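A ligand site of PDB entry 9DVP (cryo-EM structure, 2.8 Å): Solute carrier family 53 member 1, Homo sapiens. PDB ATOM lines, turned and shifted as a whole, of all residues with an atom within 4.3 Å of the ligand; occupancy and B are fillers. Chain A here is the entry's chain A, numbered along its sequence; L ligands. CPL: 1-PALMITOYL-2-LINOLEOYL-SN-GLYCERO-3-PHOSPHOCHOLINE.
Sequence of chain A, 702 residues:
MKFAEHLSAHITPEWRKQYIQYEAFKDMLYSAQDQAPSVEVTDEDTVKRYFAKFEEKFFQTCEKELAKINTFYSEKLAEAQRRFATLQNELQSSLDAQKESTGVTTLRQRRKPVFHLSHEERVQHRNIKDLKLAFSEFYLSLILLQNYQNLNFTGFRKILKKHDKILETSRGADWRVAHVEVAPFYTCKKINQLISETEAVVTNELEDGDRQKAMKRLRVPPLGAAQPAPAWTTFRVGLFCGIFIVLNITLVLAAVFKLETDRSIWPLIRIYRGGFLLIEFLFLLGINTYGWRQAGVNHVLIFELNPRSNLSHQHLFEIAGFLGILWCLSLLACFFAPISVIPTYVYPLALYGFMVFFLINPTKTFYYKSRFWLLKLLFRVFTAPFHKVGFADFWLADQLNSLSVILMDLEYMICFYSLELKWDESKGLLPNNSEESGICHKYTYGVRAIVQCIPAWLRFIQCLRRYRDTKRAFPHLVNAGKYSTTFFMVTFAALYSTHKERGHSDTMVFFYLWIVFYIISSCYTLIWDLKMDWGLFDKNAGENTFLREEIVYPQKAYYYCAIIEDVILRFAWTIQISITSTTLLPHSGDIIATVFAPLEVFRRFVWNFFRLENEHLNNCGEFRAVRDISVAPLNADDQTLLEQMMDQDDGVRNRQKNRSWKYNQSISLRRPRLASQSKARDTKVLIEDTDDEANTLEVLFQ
The backbone carbonyl oxygen (O) of Ser 309 lies close to an oxygen (O2P) of the ligand, at 2.6 Å.
N of Leu 311 sits close to O3P of the ligand, 3.2 Å away.
The side-chain hydroxyl (OG1) of Thr 289 is in hydrogen-bond range of an oxygen (O31) of the ligand, at 3.4 Å.
O1P of the ligand lies within hydrogen-bond range of OG of Ser 370 (2.6 Å).
The side-chain amide oxygen (OD1) of Asn 310 lies close to the backbone carbonyl oxygen (O) of Asn 306 (2.5 Å).
The backbone NH (N) of Ser 309 sits at hydrogen-bond distance from the side-chain amide oxygen (OD1) of Asn 306.
OG1 of Thr 289 is in hydrogen-bond range of O of Leu 285, 2.9 Å away.
Merely in contact with the ligand: Leu 278, Phe 281, Leu 282, Leu 285, His 299, Phe 303, Leu 305, Asn 306, Asn 310, Leu 316, Met 355, Val 356, Phe 358, Leu 359, Lys 369, Trp 373, Leu 374, Trp 395, Leu 396, Leu 400 and Leu 407.
Hydrophobic or aromatic side chains within 4 Å of the ligand: Leu 278, Phe 281, Leu 282, Leu 285, His 299, Phe 303, Leu 305, Leu 311, Leu 316, Met 355, Val 356, Phe 358, Leu 359, Trp 373, Leu 374, Trp 395, Leu 396, Leu 400 and Leu 407.
Within 4 Å of the ligand: Leu 278, Phe 281, Leu 282, Leu 285, Thr 289, His 299, Phe 303, Leu 305, Asn 306, Ser 309, Asn 310, Leu 311, Leu 316, Met 355, Val 356, Phe 358, Leu 359, Lys 369, Ser 370, Trp 373, Leu 374, Trp 395, Leu 396, Leu 400 and Leu 407.
The nearest printed residue that does not touch the ligand is Leu 378 (4.02 Å).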
ATOM      1  N   LEU A 278     -15.722   5.291 -18.418  1.00  0.00           N
ATOM      2  CA  LEU A 278     -15.806   6.654 -17.898  1.00  0.00           C
ATOM      3  C   LEU A 278     -17.093   6.858 -17.097  1.00  0.00           C
ATOM      4  O   LEU A 278     -17.075   7.481 -16.031  1.00  0.00           O
ATOM      5  CB  LEU A 278     -15.725   7.650 -19.050  1.00  0.00           C
ATOM      6  CG  LEU A 278     -15.305   9.074 -18.660  1.00  0.00           C
ATOM      7  CD1 LEU A 278     -13.872   9.093 -18.141  1.00  0.00           C
ATOM      8  CD2 LEU A 278     -15.450  10.020 -19.845  1.00  0.00           C
ATOM      9  N   PHE A 281     -16.707   5.107 -13.826  1.00  0.00           N
ATOM     10  CA  PHE A 281     -15.809   5.867 -12.963  1.00  0.00           C
ATOM     11  C   PHE A 281     -16.527   7.064 -12.353  1.00  0.00           C
ATOM     12  O   PHE A 281     -16.336   7.367 -11.183  1.00  0.00           O
ATOM     13  CB  PHE A 281     -14.589   6.322 -13.759  1.00  0.00           C
ATOM     14  CG  PHE A 281     -13.694   7.260 -13.008  1.00  0.00           C
ATOM     15  CD1 PHE A 281     -12.936   6.811 -11.939  1.00  0.00           C
ATOM     16  CD2 PHE A 281     -13.602   8.587 -13.370  1.00  0.00           C
ATOM     17  CE1 PHE A 281     -12.113   7.671 -11.246  1.00  0.00           C
ATOM     18  CE2 PHE A 281     -12.774   9.460 -12.678  1.00  0.00           C
ATOM     19  CZ  PHE A 281     -12.033   8.996 -11.616  1.00  0.00           C
ATOM     20  N   LEU A 282     -17.351   7.758 -13.150  1.00  0.00           N
ATOM     21  CA  LEU A 282     -18.093   8.888 -12.610  1.00  0.00           C
ATOM     22  C   LEU A 282     -19.067   8.444 -11.525  1.00  0.00           C
ATOM     23  O   LEU A 282     -19.185   9.102 -10.475  1.00  0.00           O
ATOM     24  CB  LEU A 282     -18.840   9.608 -13.730  1.00  0.00           C
ATOM     25  CG  LEU A 282     -17.978  10.393 -14.720  1.00  0.00           C
ATOM     26  CD1 LEU A 282     -18.809  10.857 -15.907  1.00  0.00           C
ATOM     27  CD2 LEU A 282     -17.319  11.585 -14.032  1.00  0.00           C
ATOM     28  N   LEU A 285     -17.166   7.549  -8.464  1.00  0.00           N
ATOM     29  CA  LEU A 285     -16.633   8.741  -7.834  1.00  0.00           C
ATOM     30  C   LEU A 285     -17.718   9.488  -7.067  1.00  0.00           C
ATOM     31  O   LEU A 285     -17.459  10.085  -6.015  1.00  0.00           O
ATOM     32  CB  LEU A 285     -15.993   9.659  -8.875  1.00  0.00           C
ATOM     33  CG  LEU A 285     -14.962  10.652  -8.338  1.00  0.00           C
ATOM     34  CD1 LEU A 285     -13.761   9.941  -7.724  1.00  0.00           C
ATOM     35  CD2 LEU A 285     -14.516  11.592  -9.433  1.00  0.00           C
ATOM     36  N   THR A 289     -17.483  10.338  -3.155  1.00  0.00           N
ATOM     37  CA  THR A 289     -17.785  11.618  -2.524  1.00  0.00           C
ATOM     38  C   THR A 289     -18.824  11.456  -1.429  1.00  0.00           C
ATOM     39  O   THR A 289     -18.697  12.055  -0.350  1.00  0.00           O
ATOM     40  CB  THR A 289     -18.265  12.617  -3.574  1.00  0.00           C
ATOM     41  OG1 THR A 289     -17.350  12.640  -4.678  1.00  0.00           O
ATOM     42  CG2 THR A 289     -18.373  14.014  -2.978  1.00  0.00           C
ATOM     43  N   TRP A 292     -17.062   9.890   1.538  1.00  0.00           N
ATOM     44  CA  TRP A 292     -16.178  10.862   2.188  1.00  0.00           C
ATOM     45  C   TRP A 292     -16.986  11.837   3.041  1.00  0.00           C
ATOM     46  O   TRP A 292     -16.597  12.163   4.165  1.00  0.00           O
ATOM     47  CB  TRP A 292     -15.366  11.622   1.140  1.00  0.00           C
ATOM     48  CG  TRP A 292     -14.404  10.765   0.363  1.00  0.00           C
ATOM     49  CD1 TRP A 292     -13.797   9.631   0.800  1.00  0.00           C
ATOM     50  CD2 TRP A 292     -13.955  10.986  -0.972  1.00  0.00           C
ATOM     51  NE1 TRP A 292     -12.987   9.123  -0.187  1.00  0.00           N
ATOM     52  CE2 TRP A 292     -13.063   9.940  -1.287  1.00  0.00           C
ATOM     53  CE3 TRP A 292     -14.210  11.966  -1.938  1.00  0.00           C
ATOM     54  CZ2 TRP A 292     -12.429   9.844  -2.524  1.00  0.00           C
ATOM     55  CZ3 TRP A 292     -13.577  11.871  -3.161  1.00  0.00           C
ATOM     56  CH2 TRP A 292     -12.690  10.819  -3.440  1.00  0.00           C
ATOM     57  N   HIS A 299     -12.455  15.843   2.221  1.00  0.00           N
ATOM     58  CA  HIS A 299     -11.881  15.796   0.887  1.00  0.00           C
ATOM     59  C   HIS A 299     -11.833  17.179   0.245  1.00  0.00           C
ATOM     60  O   HIS A 299     -11.037  17.385  -0.681  1.00  0.00           O
ATOM     61  CB  HIS A 299     -12.680  14.832   0.000  1.00  0.00           C
ATOM     62  CG  HIS A 299     -13.947  15.426  -0.535  1.00  0.00           C
ATOM     63  ND1 HIS A 299     -14.017  16.001  -1.790  1.00  0.00           N
ATOM     64  CD2 HIS A 299     -15.185  15.522  -0.005  1.00  0.00           C
ATOM     65  CE1 HIS A 299     -15.254  16.438  -2.000  1.00  0.00           C
ATOM     66  NE2 HIS A 299     -15.976  16.147  -0.933  1.00  0.00           N
ATOM     67  N   PHE A 303      -8.403  18.204  -1.537  1.00  0.00           N
ATOM     68  CA  PHE A 303      -8.408  18.550  -2.951  1.00  0.00           C
ATOM     69  C   PHE A 303      -8.262  20.047  -3.194  1.00  0.00           C
ATOM     70  O   PHE A 303      -8.238  20.475  -4.354  1.00  0.00           O
ATOM     71  CB  PHE A 303      -9.699  18.053  -3.603  1.00  0.00           C
ATOM     72  CG  PHE A 303      -9.648  16.604  -4.015  1.00  0.00           C
ATOM     73  CD1 PHE A 303      -8.979  16.225  -5.164  1.00  0.00           C
ATOM     74  CD2 PHE A 303     -10.270  15.630  -3.255  1.00  0.00           C
ATOM     75  CE1 PHE A 303      -8.921  14.897  -5.552  1.00  0.00           C
ATOM     76  CE2 PHE A 303     -10.223  14.307  -3.629  1.00  0.00           C
ATOM     77  CZ  PHE A 303      -9.548  13.940  -4.778  1.00  0.00           C
ATOM     78  N   LEU A 305     -10.354  22.541  -2.729  1.00  0.00           N
ATOM     79  CA  LEU A 305     -11.550  23.057  -3.372  1.00  0.00           C
ATOM     80  C   LEU A 305     -12.201  24.120  -2.499  1.00  0.00           C
ATOM     81  O   LEU A 305     -11.980  24.195  -1.291  1.00  0.00           O
ATOM     82  CB  LEU A 305     -12.541  21.918  -3.654  1.00  0.00           C
ATOM     83  CG  LEU A 305     -11.984  20.727  -4.430  1.00  0.00           C
ATOM     84  CD1 LEU A 305     -12.820  19.480  -4.176  1.00  0.00           C
ATOM     85  CD2 LEU A 305     -11.910  21.040  -5.923  1.00  0.00           C
ATOM     86  N   ASN A 306     -13.022  24.952  -3.130  1.00  0.00           N
ATOM     87  CA  ASN A 306     -13.683  26.041  -2.422  1.00  0.00           C
ATOM     88  C   ASN A 306     -14.721  25.454  -1.463  1.00  0.00           C
ATOM     89  O   ASN A 306     -15.660  24.791  -1.920  1.00  0.00           O
ATOM     90  CB  ASN A 306     -14.353  26.991  -3.403  1.00  0.00           C
ATOM     91  CG  ASN A 306     -15.196  28.034  -2.717  1.00  0.00           C
ATOM     92  OD1 ASN A 306     -16.372  28.213  -3.043  1.00  0.00           O
ATOM     93  ND2 ASN A 306     -14.613  28.737  -1.749  1.00  0.00           N
ATOM     94  N   SER A 309     -18.609  26.200  -2.249  1.00  0.00           N
ATOM     95  CA  SER A 309     -19.276  25.648  -3.431  1.00  0.00           C
ATOM     96  C   SER A 309     -18.607  24.312  -3.735  1.00  0.00           C
ATOM     97  O   SER A 309     -17.559  24.258  -4.397  1.00  0.00           O
ATOM     98  CB  SER A 309     -19.201  26.600  -4.611  1.00  0.00           C
ATOM     99  OG  SER A 309     -20.231  26.335  -5.546  1.00  0.00           O
ATOM    100  N   ASN A 310     -19.213  23.229  -3.247  1.00  0.00           N
ATOM    101  CA  ASN A 310     -18.703  21.870  -3.445  1.00  0.00           C
ATOM    102  C   ASN A 310     -19.675  21.088  -4.319  1.00  0.00           C
ATOM    103  O   ASN A 310     -20.883  21.062  -4.038  1.00  0.00           O
ATOM    104  CB  ASN A 310     -18.514  21.152  -2.109  1.00  0.00           C
ATOM    105  CG  ASN A 310     -17.688  21.966  -1.131  1.00  0.00           C
ATOM    106  OD1 ASN A 310     -16.631  22.495  -1.471  1.00  0.00           O
ATOM    107  ND2 ASN A 310     -18.177  22.069   0.107  1.00  0.00           N
ATOM    108  N   LEU A 311     -19.156  20.474  -5.376  1.00  0.00           N
ATOM    109  CA  LEU A 311     -19.964  19.621  -6.238  1.00  0.00           C
ATOM    110  C   LEU A 311     -20.369  18.369  -5.457  1.00  0.00           C
ATOM    111  O   LEU A 311     -19.534  17.513  -5.178  1.00  0.00           O
ATOM    112  CB  LEU A 311     -19.195  19.252  -7.501  1.00  0.00           C
ATOM    113  CG  LEU A 311     -19.929  18.391  -8.522  1.00  0.00           C
ATOM    114  CD1 LEU A 311     -20.353  19.218  -9.726  1.00  0.00           C
ATOM    115  CD2 LEU A 311     -19.072  17.219  -8.948  1.00  0.00           C
ATOM    116  N   LEU A 316     -22.490  14.528  -9.297  1.00  0.00           N
ATOM    117  CA  LEU A 316     -21.705  13.502  -9.979  1.00  0.00           C
ATOM    118  C   LEU A 316     -22.603  12.391 -10.505  1.00  0.00           C
ATOM    119  O   LEU A 316     -22.418  11.927 -11.636  1.00  0.00           O
ATOM    120  CB  LEU A 316     -20.655  12.928  -9.017  1.00  0.00           C
ATOM    121  CG  LEU A 316     -19.266  13.562  -9.101  1.00  0.00           C
ATOM    122  CD1 LEU A 316     -18.493  13.309  -7.810  1.00  0.00           C
ATOM    123  CD2 LEU A 316     -18.504  13.035 -10.296  1.00  0.00           C
ATOM    124  N   ILE A 319     -24.410  13.699 -13.623  1.00  0.00           N
ATOM    125  CA  ILE A 319     -23.543  13.726 -14.801  1.00  0.00           C
ATOM    126  C   ILE A 319     -23.329  12.308 -15.326  1.00  0.00           C
ATOM    127  O   ILE A 319     -23.387  12.055 -16.533  1.00  0.00           O
ATOM    128  CB  ILE A 319     -22.202  14.415 -14.464  1.00  0.00           C
ATOM    129  CG1 ILE A 319     -22.439  15.881 -14.104  1.00  0.00           C
ATOM    130  CG2 ILE A 319     -21.242  14.303 -15.640  1.00  0.00           C
ATOM    131  CD1 ILE A 319     -21.272  16.532 -13.386  1.00  0.00           C
ATOM    132  N   LEU A 323     -24.463  10.945 -19.039  1.00  0.00           N
ATOM    133  CA  LEU A 323     -23.479  10.347 -19.943  1.00  0.00           C
ATOM    134  C   LEU A 323     -23.856   8.906 -20.274  1.00  0.00           C
ATOM    135  O   LEU A 323     -23.701   8.470 -21.421  1.00  0.00           O
ATOM    136  CB  LEU A 323     -22.087  10.416 -19.315  1.00  0.00           C
ATOM    137  CG  LEU A 323     -21.395  11.790 -19.227  1.00  0.00           C
ATOM    138  CD1 LEU A 323     -19.889  11.620 -19.364  1.00  0.00           C
ATOM    139  CD2 LEU A 323     -21.913  12.782 -20.257  1.00  0.00           C
ATOM    140  N   MET A 355     -19.428  14.550 -25.366  1.00  0.00           N
ATOM    141  CA  MET A 355     -18.743  14.550 -24.074  1.00  0.00           C
ATOM    142  C   MET A 355     -17.579  15.536 -24.089  1.00  0.00           C
ATOM    143  O   MET A 355     -17.441  16.360 -23.185  1.00  0.00           O
ATOM    144  CB  MET A 355     -18.257  13.144 -23.734  1.00  0.00           C
ATOM    145  CG  MET A 355     -19.373  12.099 -23.693  1.00  0.00           C
ATOM    146  SD  MET A 355     -18.865  10.438 -23.202  1.00  0.00           S
ATOM    147  CE  MET A 355     -17.103  10.623 -22.939  1.00  0.00           C
ATOM    148  N   VAL A 356     -16.763  15.486 -25.147  1.00  0.00           N
ATOM    149  CA  VAL A 356     -15.677  16.451 -25.272  1.00  0.00           C
ATOM    150  C   VAL A 356     -16.248  17.865 -25.262  1.00  0.00           C
ATOM    151  O   VAL A 356     -15.817  18.717 -24.485  1.00  0.00           O
ATOM    152  CB  VAL A 356     -14.857  16.175 -26.542  1.00  0.00           C
ATOM    153  CG1 VAL A 356     -13.851  17.288 -26.783  1.00  0.00           C
ATOM    154  CG2 VAL A 356     -14.152  14.834 -26.440  1.00  0.00           C
ATOM    155  N   PHE A 358     -18.966  18.717 -24.038  1.00  0.00           N
ATOM    156  CA  PHE A 358     -19.477  18.937 -22.692  1.00  0.00           C
ATOM    157  C   PHE A 358     -18.363  19.374 -21.750  1.00  0.00           C
ATOM    158  O   PHE A 358     -18.568  20.253 -20.910  1.00  0.00           O
ATOM    159  CB  PHE A 358     -20.171  17.684 -22.167  1.00  0.00           C
ATOM    160  CG  PHE A 358     -20.753  17.843 -20.795  1.00  0.00           C
ATOM    161  CD1 PHE A 358     -22.018  18.380 -20.620  1.00  0.00           C
ATOM    162  CD2 PHE A 358     -20.042  17.446 -19.673  1.00  0.00           C
ATOM    163  CE1 PHE A 358     -22.564  18.530 -19.366  1.00  0.00           C
ATOM    164  CE2 PHE A 358     -20.581  17.586 -18.411  1.00  0.00           C
ATOM    165  CZ  PHE A 358     -21.842  18.128 -18.257  1.00  0.00           C
ATOM    166  N   LEU A 359     -17.186  18.768 -21.885  1.00  0.00           N
ATOM    167  CA  LEU A 359     -16.087  19.088 -20.969  1.00  0.00           C
ATOM    168  C   LEU A 359     -15.473  20.446 -21.281  1.00  0.00           C
ATOM    169  O   LEU A 359     -15.155  21.208 -20.366  1.00  0.00           O
ATOM    170  CB  LEU A 359     -15.019  17.983 -21.031  1.00  0.00           C
ATOM    171  CG  LEU A 359     -13.759  18.210 -20.195  1.00  0.00           C
ATOM    172  CD1 LEU A 359     -14.107  18.323 -18.716  1.00  0.00           C
ATOM    173  CD2 LEU A 359     -12.757  17.101 -20.431  1.00  0.00           C
ATOM    174  N   LYS A 369     -17.929  25.901 -13.446  1.00  0.00           N
ATOM    175  CA  LYS A 369     -16.801  26.062 -12.531  1.00  0.00           C
ATOM    176  C   LYS A 369     -16.062  24.738 -12.342  1.00  0.00           C
ATOM    177  O   LYS A 369     -14.829  24.678 -12.420  1.00  0.00           O
ATOM    178  CB  LYS A 369     -17.284  26.601 -11.186  1.00  0.00           C
ATOM    179  CG  LYS A 369     -17.892  27.993 -11.270  1.00  0.00           C
ATOM    180  CD  LYS A 369     -17.856  28.702  -9.922  1.00  0.00           C
ATOM    181  CE  LYS A 369     -16.565  29.481  -9.739  1.00  0.00           C
ATOM    182  NZ  LYS A 369     -16.475  30.636 -10.663  1.00  0.00           N
ATOM    183  N   SER A 370     -16.814  23.662 -12.082  1.00  0.00           N
ATOM    184  CA  SER A 370     -16.199  22.353 -11.908  1.00  0.00           C
ATOM    185  C   SER A 370     -15.496  21.904 -13.186  1.00  0.00           C
ATOM    186  O   SER A 370     -14.405  21.329 -13.136  1.00  0.00           O
ATOM    187  CB  SER A 370     -17.263  21.335 -11.496  1.00  0.00           C
ATOM    188  OG  SER A 370     -18.223  21.930 -10.640  1.00  0.00           O
ATOM    189  N   TRP A 373     -12.253  23.796 -13.510  1.00  0.00           N
ATOM    190  CA  TRP A 373     -11.279  23.247 -12.560  1.00  0.00           C
ATOM    191  C   TRP A 373     -10.707  21.928 -13.075  1.00  0.00           C
ATOM    192  O   TRP A 373      -9.491  21.700 -13.000  1.00  0.00           O
ATOM    193  CB  TRP A 373     -11.945  23.057 -11.195  1.00  0.00           C
ATOM    194  CG  TRP A 373     -11.021  22.537 -10.128  1.00  0.00           C
ATOM    195  CD1 TRP A 373     -10.239  23.277  -9.293  1.00  0.00           C
ATOM    196  CD2 TRP A 373     -10.803  21.169  -9.776  1.00  0.00           C
ATOM    197  NE1 TRP A 373      -9.536  22.458  -8.449  1.00  0.00           N
ATOM    198  CE2 TRP A 373      -9.869  21.153  -8.725  1.00  0.00           C
ATOM    199  CE3 TRP A 373     -11.304  19.949 -10.248  1.00  0.00           C
ATOM    200  CZ2 TRP A 373      -9.424  19.973  -8.132  1.00  0.00           C
ATOM    201  CZ3 TRP A 373     -10.855  18.776  -9.663  1.00  0.00           C
ATOM    202  CH2 TRP A 373      -9.925  18.800  -8.619  1.00  0.00           C
ATOM    203  N   LEU A 374     -11.565  21.062 -13.606  1.00  0.00           N
ATOM    204  CA  LEU A 374     -11.087  19.799 -14.157  1.00  0.00           C
ATOM    205  C   LEU A 374     -10.168  20.019 -15.352  1.00  0.00           C
ATOM    206  O   LEU A 374      -9.161  19.317 -15.508  1.00  0.00           O
ATOM    207  CB  LEU A 374     -12.278  18.914 -14.558  1.00  0.00           C
ATOM    208  CG  LEU A 374     -11.908  17.566 -15.176  1.00  0.00           C
ATOM    209  CD1 LEU A 374     -10.987  16.785 -14.257  1.00  0.00           C
ATOM    210  CD2 LEU A 374     -13.157  16.761 -15.504  1.00  0.00           C
ATOM    211  N   LEU A 378      -6.353  18.789 -15.561  1.00  0.00           N
ATOM    212  CA  LEU A 378      -5.885  17.927 -16.635  1.00  0.00           C
ATOM    213  C   LEU A 378      -4.690  18.541 -17.345  1.00  0.00           C
ATOM    214  O   LEU A 378      -3.711  17.849 -17.659  1.00  0.00           O
ATOM    215  CB  LEU A 378      -7.011  17.657 -17.632  1.00  0.00           C
ATOM    216  CG  LEU A 378      -8.045  16.611 -17.204  1.00  0.00           C
ATOM    217  CD1 LEU A 378      -9.366  16.849 -17.909  1.00  0.00           C
ATOM    218  CD2 LEU A 378      -7.525  15.208 -17.493  1.00  0.00           C
ATOM    219  N   TRP A 395      -3.597  12.652  -7.700  1.00  0.00           N
ATOM    220  CA  TRP A 395      -4.817  11.845  -7.665  1.00  0.00           C
ATOM    221  C   TRP A 395      -5.374  11.643  -9.064  1.00  0.00           C
ATOM    222  O   TRP A 395      -5.772  10.527  -9.428  1.00  0.00           O
ATOM    223  CB  TRP A 395      -5.837  12.512  -6.758  1.00  0.00           C
ATOM    224  CG  TRP A 395      -7.101  11.724  -6.599  1.00  0.00           C
ATOM    225  CD1 TRP A 395      -7.356  10.770  -5.669  1.00  0.00           C
ATOM    226  CD2 TRP A 395      -8.282  11.840  -7.405  1.00  0.00           C
ATOM    227  NE1 TRP A 395      -8.628  10.268  -5.839  1.00  0.00           N
ATOM    228  CE2 TRP A 395      -9.209  10.902  -6.904  1.00  0.00           C
ATOM    229  CE3 TRP A 395      -8.631  12.629  -8.498  1.00  0.00           C
ATOM    230  CZ2 TRP A 395     -10.479  10.751  -7.452  1.00  0.00           C
ATOM    231  CZ3 TRP A 395      -9.894  12.467  -9.052  1.00  0.00           C
ATOM    232  CH2 TRP A 395     -10.796  11.541  -8.529  1.00  0.00           C
ATOM    233  N   LEU A 396      -5.417  12.710  -9.872  1.00  0.00           N
ATOM    234  CA  LEU A 396      -5.936  12.577 -11.222  1.00  0.00           C
ATOM    235  C   LEU A 396      -5.005  11.733 -12.100  1.00  0.00           C
ATOM    236  O   LEU A 396      -5.465  10.978 -12.960  1.00  0.00           O
ATOM    237  CB  LEU A 396      -6.139  13.960 -11.850  1.00  0.00           C
ATOM    238  CG  LEU A 396      -6.913  13.976 -13.169  1.00  0.00           C
ATOM    239  CD1 LEU A 396      -8.353  13.525 -12.960  1.00  0.00           C
ATOM    240  CD2 LEU A 396      -6.868  15.352 -13.805  1.00  0.00           C
ATOM    241  N   LEU A 400      -6.067   8.374 -14.083  1.00  0.00           N
ATOM    242  CA  LEU A 400      -5.709   8.072 -15.456  1.00  0.00           C
ATOM    243  C   LEU A 400      -4.990   6.732 -15.559  1.00  0.00           C
ATOM    244  O   LEU A 400      -5.243   5.942 -16.469  1.00  0.00           O
ATOM    245  CB  LEU A 400      -4.832   9.185 -16.037  1.00  0.00           C
ATOM    246  CG  LEU A 400      -5.482  10.500 -16.461  1.00  0.00           C
ATOM    247  CD1 LEU A 400      -4.696  11.132 -17.605  1.00  0.00           C
ATOM    248  CD2 LEU A 400      -6.948  10.348 -16.857  1.00  0.00           C
ATOM    249  N   LEU A 407      -7.447   5.387 -23.186  1.00  0.00           N
ATOM    250  CA  LEU A 407      -6.407   5.780 -24.132  1.00  0.00           C
ATOM    251  C   LEU A 407      -6.092   4.654 -25.100  1.00  0.00           C
ATOM    252  O   LEU A 407      -5.889   4.882 -26.300  1.00  0.00           O
ATOM    253  CB  LEU A 407      -5.146   6.199 -23.380  1.00  0.00           C
ATOM    254  CG  LEU A 407      -4.925   7.706 -23.216  1.00  0.00           C
ATOM    255  CD1 LEU A 407      -6.169   8.382 -22.641  1.00  0.00           C
ATOM    256  CD2 LEU A 407      -3.715   7.977 -22.335  1.00  0.00           C
HETATM  257  C1  CPL L   1     -15.582  19.665  -6.263  1.00  0.00           C
HETATM  258  C2  CPL L   1     -15.463  18.172  -6.685  1.00  0.00           C
HETATM  259  C3  CPL L   1     -14.624  18.111  -7.997  1.00  0.00           C
HETATM  260  C4  CPL L   1     -14.294  22.995  -7.881  1.00  0.00           C
HETATM  261  C5  CPL L   1     -14.789  24.249  -8.571  1.00  0.00           C
HETATM  262  C6  CPL L   1     -12.737  25.338  -7.534  1.00  0.00           C
HETATM  263  C7  CPL L   1     -15.002  25.509  -6.511  1.00  0.00           C
HETATM  264  C8  CPL L   1     -14.501  26.749  -8.583  1.00  0.00           C
HETATM  265  C11 CPL L   1     -14.764  19.226 -10.101  1.00  0.00           C
HETATM  266  C12 CPL L   1     -14.901  18.468 -11.396  1.00  0.00           C
HETATM  267  C13 CPL L   1     -15.676  17.148 -11.207  1.00  0.00           C
HETATM  268  C14 CPL L   1     -15.884  16.374 -12.520  1.00  0.00           C
HETATM  269  C15 CPL L   1     -17.119  16.821 -13.326  1.00  0.00           C
HETATM  270  C16 CPL L   1     -17.370  15.935 -14.559  1.00  0.00           C
HETATM  271  C17 CPL L   1     -17.206  16.656 -15.919  1.00  0.00           C
HETATM  272  C18 CPL L   1     -17.472  15.738 -17.131  1.00  0.00           C
HETATM  273  C19 CPL L   1     -16.660  14.420 -17.172  1.00  0.00           C
HETATM  274  C20 CPL L   1     -16.470  13.752 -18.551  1.00  0.00           C
HETATM  275  C21 CPL L   1     -15.219  14.149 -19.358  1.00  0.00           C
HETATM  276  C22 CPL L   1     -15.374  13.874 -20.867  1.00  0.00           C
HETATM  277  C23 CPL L   1     -14.075  13.558 -21.592  1.00  0.00           C
HETATM  278  C24 CPL L   1     -14.293  12.949 -22.989  1.00  0.00           C
HETATM  279  C25 CPL L   1     -13.601  11.590 -23.135  1.00  0.00           C
HETATM  280  C26 CPL L   1     -12.116  11.758 -23.390  1.00  0.00           C
HETATM  281  C31 CPL L   1     -14.824  16.028  -5.719  1.00  0.00           C
HETATM  282  C32 CPL L   1     -13.472  15.349  -5.516  1.00  0.00           C
HETATM  283  C33 CPL L   1     -12.536  15.555  -6.731  1.00  0.00           C
HETATM  284  C34 CPL L   1     -12.947  14.684  -7.924  1.00  0.00           C
HETATM  285  C35 CPL L   1     -12.412  15.207  -9.264  1.00  0.00           C
HETATM  286  C36 CPL L   1     -12.728  14.257 -10.428  1.00  0.00           C
HETATM  287  C37 CPL L   1     -12.248  14.750 -11.791  1.00  0.00           C
HETATM  288  C38 CPL L   1     -12.200  13.645 -12.860  1.00  0.00           C
HETATM  289  C39 CPL L   1     -13.536  13.475 -13.510  1.00  0.00           C
HETATM  290  C40 CPL L   1     -13.766  13.241 -14.791  1.00  0.00           C
HETATM  291  C41 CPL L   1     -12.718  13.123 -15.849  1.00  0.00           C
HETATM  292  C42 CPL L   1     -11.901  11.881 -15.651  1.00  0.00           C
HETATM  293  C43 CPL L   1     -10.854  11.535 -16.390  1.00  0.00           C
HETATM  294  C44 CPL L   1     -10.320  12.314 -17.546  1.00  0.00           C
HETATM  295  C45 CPL L   1     -10.951  11.898 -18.886  1.00  0.00           C
HETATM  296  C46 CPL L   1     -10.096  10.849 -19.614  1.00  0.00           C
HETATM  297  C47 CPL L   1      -8.789  11.447 -20.147  1.00  0.00           C
HETATM  298  C48 CPL L   1      -8.314  10.703 -21.380  1.00  0.00           C
HETATM  299  N   CPL L   1     -14.225  25.459  -7.812  1.00  0.00           N
HETATM  300  O2  CPL L   1     -14.834  17.387  -5.662  1.00  0.00           O
HETATM  301  O3  CPL L   1     -15.405  18.662  -9.042  1.00  0.00           O
HETATM  302  O11 CPL L   1     -14.156  20.259  -9.971  1.00  0.00           O
HETATM  303  O31 CPL L   1     -15.817  15.359  -5.909  1.00  0.00           O
HETATM  304  O1P CPL L   1     -17.741  22.218  -8.100  1.00  0.00           O
HETATM  305  O2P CPL L   1     -16.271  22.457  -5.807  1.00  0.00           O
HETATM  306  O3P CPL L   1     -16.489  20.264  -7.098  1.00  0.00           O
HETATM  307  O4P CPL L   1     -15.209  22.008  -8.178  1.00  0.00           O
HETATM  308  P   CPL L   1     -16.602  21.997  -7.179  1.00  0.00           P
